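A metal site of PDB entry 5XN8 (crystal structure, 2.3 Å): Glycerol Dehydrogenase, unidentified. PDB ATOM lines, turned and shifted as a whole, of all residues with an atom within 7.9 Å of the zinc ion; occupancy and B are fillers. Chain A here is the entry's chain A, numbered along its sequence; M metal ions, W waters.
OD1 of Asp 121 touches the zinc ion (3.7 Å).
Four residues have an atom within 4 Å of the zinc ion: Asp 121, Asp 171, His 254 and His 271.
The nearest printed residue that does not touch the zinc ion is Val 275 (4.3 Å).
The side-chain carboxylate (OD2) of Asp 171 lies within hydrogen-bond range of the backbone NH (N) of Asp 121 (3.2 Å).
The backbone carbonyl oxygen (O) of Asp 171 lies within hydrogen-bond range of the side-chain hydroxyl (OG) of Ser 174 (2.8 Å).
The side-chain carboxylate (OD2) of Asp 171 is in hydrogen-bond range of the side-chain hydroxyl (OG1) of Thr 120, at 3.3 Å.
A ring nitrogen (ND1) of His 254 sits at hydrogen-bond distance from the side-chain carboxylate (OE1) of Glu 178 (2.8 Å).
The side-chain hydroxyl (OG) of Ser 241 is in hydrogen-bond range of the side-chain carboxylate (OD2) of Asp 121, 2.6 Å away.
A ring nitrogen (NE2) of His 257 sits at hydrogen-bond distance from a ring nitrogen (ND1) of His 271.
The zinc ion is bound by OD1 of Asp 171, at 2.1 Å.
Water W1 binds the zinc ion, 2.1 Å away.
The zinc ion is bound by a ring nitrogen (NE2) of His 254, at 2.2 Å.
The zinc ion is bound by a ring nitrogen (NE2) of His 271 (2.2 Å).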
ATOM      1  N   SER A 119       8.434  -6.888  18.463  1.00  0.00           N
ATOM      2  CA  SER A 119       7.833  -8.173  18.879  1.00  0.00           C
ATOM      3  C   SER A 119       8.556  -8.923  19.992  1.00  0.00           C
ATOM      4  O   SER A 119       8.042  -9.921  20.491  1.00  0.00           O
ATOM      5  CB  SER A 119       7.700  -9.080  17.653  1.00  0.00           C
ATOM      6  OG  SER A 119       8.975  -9.315  17.075  1.00  0.00           O
ATOM      7  N   THR A 120       9.753  -8.458  20.357  1.00  0.00           N
ATOM      8  CA  THR A 120      10.547  -9.027  21.443  1.00  0.00           C
ATOM      9  C   THR A 120      11.286  -7.915  22.167  1.00  0.00           C
ATOM     10  O   THR A 120      11.327  -6.777  21.685  1.00  0.00           O
ATOM     11  CB  THR A 120      11.568 -10.082  20.943  1.00  0.00           C
ATOM     12  OG1 THR A 120      12.275 -10.623  22.055  1.00  0.00           O
ATOM     13  CG2 THR A 120      12.545  -9.499  19.892  1.00  0.00           C
ATOM     14  N   ASP A 121      11.872  -8.251  23.311  1.00  0.00           N
ATOM     15  CA  ASP A 121      12.701  -7.328  24.100  1.00  0.00           C
ATOM     16  C   ASP A 121      14.199  -7.657  23.982  1.00  0.00           C
ATOM     17  O   ASP A 121      15.023  -7.134  24.730  1.00  0.00           O
ATOM     18  CB  ASP A 121      12.234  -7.279  25.565  1.00  0.00           C
ATOM     19  CG  ASP A 121      12.274  -8.635  26.268  1.00  0.00           C
ATOM     20  OD1 ASP A 121      12.641  -9.652  25.631  1.00  0.00           O
ATOM     21  OD2 ASP A 121      11.931  -8.659  27.482  1.00  0.00           O
ATOM     22  N   ALA A 122      14.534  -8.499  22.992  1.00  0.00           N
ATOM     23  CA  ALA A 122      15.906  -8.865  22.676  1.00  0.00           C
ATOM     24  C   ALA A 122      16.790  -7.699  22.189  1.00  0.00           C
ATOM     25  O   ALA A 122      17.958  -7.669  22.570  1.00  0.00           O
ATOM     26  CB  ALA A 122      15.930  -9.987  21.643  1.00  0.00           C
ATOM     27  N   SER A 167       2.375  -9.840  20.073  1.00  0.00           N
ATOM     28  CA  SER A 167       3.340 -10.800  20.637  1.00  0.00           C
ATOM     29  C   SER A 167       4.396 -10.087  21.465  1.00  0.00           C
ATOM     30  O   SER A 167       4.837 -10.612  22.495  1.00  0.00           O
ATOM     31  CB  SER A 167       4.007 -11.630  19.530  1.00  0.00           C
ATOM     32  OG  SER A 167       4.718 -12.713  20.097  1.00  0.00           O
ATOM     33  N   GLY A 168       4.795  -8.889  21.028  1.00  0.00           N
ATOM     34  CA  GLY A 168       5.706  -8.041  21.800  1.00  0.00           C
ATOM     35  C   GLY A 168       5.174  -7.626  23.151  1.00  0.00           C
ATOM     36  O   GLY A 168       5.939  -7.542  24.126  1.00  0.00           O
ATOM     37  N   GLY A 170       2.965  -9.432  24.806  1.00  0.00           N
ATOM     38  CA  GLY A 170       2.979 -10.700  25.547  1.00  0.00           C
ATOM     39  C   GLY A 170       4.316 -10.996  26.183  1.00  0.00           C
ATOM     40  O   GLY A 170       4.373 -11.531  27.280  1.00  0.00           O
ATOM     41  N   ASP A 171       5.401 -10.667  25.476  1.00  0.00           N
ATOM     42  CA  ASP A 171       6.772 -10.839  25.981  1.00  0.00           C
ATOM     43  C   ASP A 171       7.055  -9.846  27.107  1.00  0.00           C
ATOM     44  O   ASP A 171       7.765 -10.153  28.068  1.00  0.00           O
ATOM     45  CB  ASP A 171       7.777 -10.652  24.832  1.00  0.00           C
ATOM     46  CG  ASP A 171       9.184 -11.149  25.151  1.00  0.00           C
ATOM     47  OD1 ASP A 171       9.371 -12.118  25.919  1.00  0.00           O
ATOM     48  OD2 ASP A 171      10.136 -10.579  24.589  1.00  0.00           O
ATOM     49  N   ALA A 172       6.489  -8.657  26.963  1.00  0.00           N
ATOM     50  CA  ALA A 172       6.696  -7.551  27.900  1.00  0.00           C
ATOM     51  C   ALA A 172       5.875  -7.691  29.184  1.00  0.00           C
ATOM     52  O   ALA A 172       6.331  -7.301  30.264  1.00  0.00           O
ATOM     53  CB  ALA A 172       6.380  -6.226  27.217  1.00  0.00           C
ATOM     54  N   SER A 174       5.330 -10.315  30.855  1.00  0.00           N
ATOM     55  CA  SER A 174       6.066 -11.173  31.795  1.00  0.00           C
ATOM     56  C   SER A 174       7.135 -10.475  32.623  1.00  0.00           C
ATOM     57  O   SER A 174       7.632 -11.048  33.578  1.00  0.00           O
ATOM     58  CB  SER A 174       6.784 -12.259  31.016  1.00  0.00           C
ATOM     59  OG  SER A 174       7.917 -11.713  30.358  1.00  0.00           O
ATOM     60  N   THR A 175       7.534  -9.275  32.229  1.00  0.00           N
ATOM     61  CA  THR A 175       8.762  -8.675  32.759  1.00  0.00           C
ATOM     62  C   THR A 175       8.654  -8.316  34.223  1.00  0.00           C
ATOM     63  O   THR A 175       9.527  -8.681  35.011  1.00  0.00           O
ATOM     64  CB  THR A 175       9.175  -7.441  31.924  1.00  0.00           C
ATOM     65  OG1 THR A 175       9.345  -7.861  30.562  1.00  0.00           O
ATOM     66  CG2 THR A 175      10.475  -6.856  32.413  1.00  0.00           C
ATOM     67  N   GLU A 178       8.380 -11.694  36.555  1.00  0.00           N
ATOM     68  CA  GLU A 178       9.662 -12.393  36.668  1.00  0.00           C
ATOM     69  C   GLU A 178      10.737 -11.543  37.335  1.00  0.00           C
ATOM     70  O   GLU A 178      11.583 -12.063  38.087  1.00  0.00           O
ATOM     71  CB  GLU A 178      10.158 -12.802  35.281  1.00  0.00           C
ATOM     72  CG  GLU A 178       9.228 -13.792  34.571  1.00  0.00           C
ATOM     73  CD  GLU A 178       9.765 -14.202  33.228  1.00  0.00           C
ATOM     74  OE1 GLU A 178       9.684 -13.417  32.263  1.00  0.00           O
ATOM     75  OE2 GLU A 178      10.254 -15.340  33.114  1.00  0.00           O
ATOM     76  N   SER A 241      11.099  -3.390  28.886  1.00  0.00           N
ATOM     77  CA  SER A 241      11.111  -4.843  29.047  1.00  0.00           C
ATOM     78  C   SER A 241      12.526  -5.379  28.957  1.00  0.00           C
ATOM     79  O   SER A 241      12.898  -6.295  29.697  1.00  0.00           O
ATOM     80  CB  SER A 241      10.196  -5.512  28.014  1.00  0.00           C
ATOM     81  OG  SER A 241      10.124  -6.919  28.201  1.00  0.00           O
ATOM     82  N   PHE A 245      14.303  -7.468  31.952  1.00  0.00           N
ATOM     83  CA  PHE A 245      14.652  -8.904  32.003  1.00  0.00           C
ATOM     84  C   PHE A 245      16.149  -9.132  32.256  1.00  0.00           C
ATOM     85  O   PHE A 245      16.524 -10.030  33.010  1.00  0.00           O
ATOM     86  CB  PHE A 245      14.122  -9.668  30.766  1.00  0.00           C
ATOM     87  CG  PHE A 245      15.121  -9.837  29.631  1.00  0.00           C
ATOM     88  CD1 PHE A 245      16.052 -10.857  29.660  1.00  0.00           C
ATOM     89  CD2 PHE A 245      15.084  -8.989  28.530  1.00  0.00           C
ATOM     90  CE1 PHE A 245      16.968 -11.019  28.622  1.00  0.00           C
ATOM     91  CE2 PHE A 245      15.985  -9.137  27.492  1.00  0.00           C
ATOM     92  CZ  PHE A 245      16.928 -10.158  27.528  1.00  0.00           C
ATOM     93  N   LEU A 250      14.858 -12.985  34.694  1.00  0.00           N
ATOM     94  CA  LEU A 250      13.855 -13.924  34.200  1.00  0.00           C
ATOM     95  C   LEU A 250      13.550 -14.969  35.277  1.00  0.00           C
ATOM     96  O   LEU A 250      14.358 -15.226  36.159  1.00  0.00           O
ATOM     97  CB  LEU A 250      14.385 -14.698  32.977  1.00  0.00           C
ATOM     98  CG  LEU A 250      14.851 -13.922  31.757  1.00  0.00           C
ATOM     99  CD1 LEU A 250      15.620 -14.841  30.817  1.00  0.00           C
ATOM    100  CD2 LEU A 250      13.657 -13.308  31.040  1.00  0.00           C
ATOM    101  N   HIS A 254       9.407 -17.602  31.399  1.00  0.00           N
ATOM    102  CA  HIS A 254      10.348 -17.883  30.289  1.00  0.00           C
ATOM    103  C   HIS A 254      10.890 -19.313  30.314  1.00  0.00           C
ATOM    104  O   HIS A 254      11.165 -19.894  29.271  1.00  0.00           O
ATOM    105  CB  HIS A 254      11.479 -16.843  30.298  1.00  0.00           C
ATOM    106  CG  HIS A 254      11.204 -15.656  29.429  1.00  0.00           C
ATOM    107  ND1 HIS A 254      10.501 -14.544  29.846  1.00  0.00           N
ATOM    108  CD2 HIS A 254      11.607 -15.392  28.164  1.00  0.00           C
ATOM    109  CE1 HIS A 254      10.426 -13.685  28.850  1.00  0.00           C
ATOM    110  NE2 HIS A 254      11.106 -14.162  27.829  1.00  0.00           N
ATOM    111  N   HIS A 257       7.965 -21.168  28.771  1.00  0.00           N
ATOM    112  CA  HIS A 257       8.109 -20.958  27.328  1.00  0.00           C
ATOM    113  C   HIS A 257       9.079 -21.943  26.712  1.00  0.00           C
ATOM    114  O   HIS A 257       8.797 -22.510  25.668  1.00  0.00           O
ATOM    115  CB  HIS A 257       8.567 -19.514  27.010  1.00  0.00           C
ATOM    116  CG  HIS A 257       9.211 -19.356  25.667  1.00  0.00           C
ATOM    117  ND1 HIS A 257      10.523 -19.720  25.421  1.00  0.00           N
ATOM    118  CD2 HIS A 257       8.727 -18.893  24.497  1.00  0.00           C
ATOM    119  CE1 HIS A 257      10.802 -19.482  24.148  1.00  0.00           C
ATOM    120  NE2 HIS A 257       9.729 -18.979  23.572  1.00  0.00           N
ATOM    121  N   HIS A 271       7.331 -16.209  20.020  1.00  0.00           N
ATOM    122  CA  HIS A 271       7.989 -16.170  21.335  1.00  0.00           C
ATOM    123  C   HIS A 271       7.119 -15.568  22.441  1.00  0.00           C
ATOM    124  O   HIS A 271       6.892 -16.188  23.488  1.00  0.00           O
ATOM    125  CB  HIS A 271       9.301 -15.380  21.201  1.00  0.00           C
ATOM    126  CG  HIS A 271      10.068 -15.251  22.472  1.00  0.00           C
ATOM    127  ND1 HIS A 271      10.760 -16.296  23.051  1.00  0.00           N
ATOM    128  CD2 HIS A 271      10.293 -14.177  23.276  1.00  0.00           C
ATOM    129  CE1 HIS A 271      11.359 -15.878  24.153  1.00  0.00           C
ATOM    130  NE2 HIS A 271      11.086 -14.596  24.306  1.00  0.00           N
ATOM    131  N   GLY A 272       6.626 -14.353  22.213  1.00  0.00           N
ATOM    132  CA  GLY A 272       5.893 -13.620  23.223  1.00  0.00           C
ATOM    133  C   GLY A 272       4.498 -14.118  23.544  1.00  0.00           C
ATOM    134  O   GLY A 272       4.003 -13.919  24.641  1.00  0.00           O
ATOM    135  N   VAL A 275       5.018 -16.808  26.016  1.00  0.00           N
ATOM    136  CA  VAL A 275       5.398 -16.134  27.268  1.00  0.00           C
ATOM    137  C   VAL A 275       4.163 -15.572  27.989  1.00  0.00           C
ATOM    138  O   VAL A 275       4.099 -15.587  29.228  1.00  0.00           O
ATOM    139  CB  VAL A 275       6.436 -15.017  26.998  1.00  0.00           C
ATOM    140  CG1 VAL A 275       6.658 -14.121  28.212  1.00  0.00           C
ATOM    141  CG2 VAL A 275       7.766 -15.597  26.555  1.00  0.00           C
HETATM  142 ZN    ZN M   1      11.222 -13.077  25.935  1.00  0.00          ZN
HETATM  143  O   HOH W   1      13.133 -14.012  26.092  1.00  0.00           O
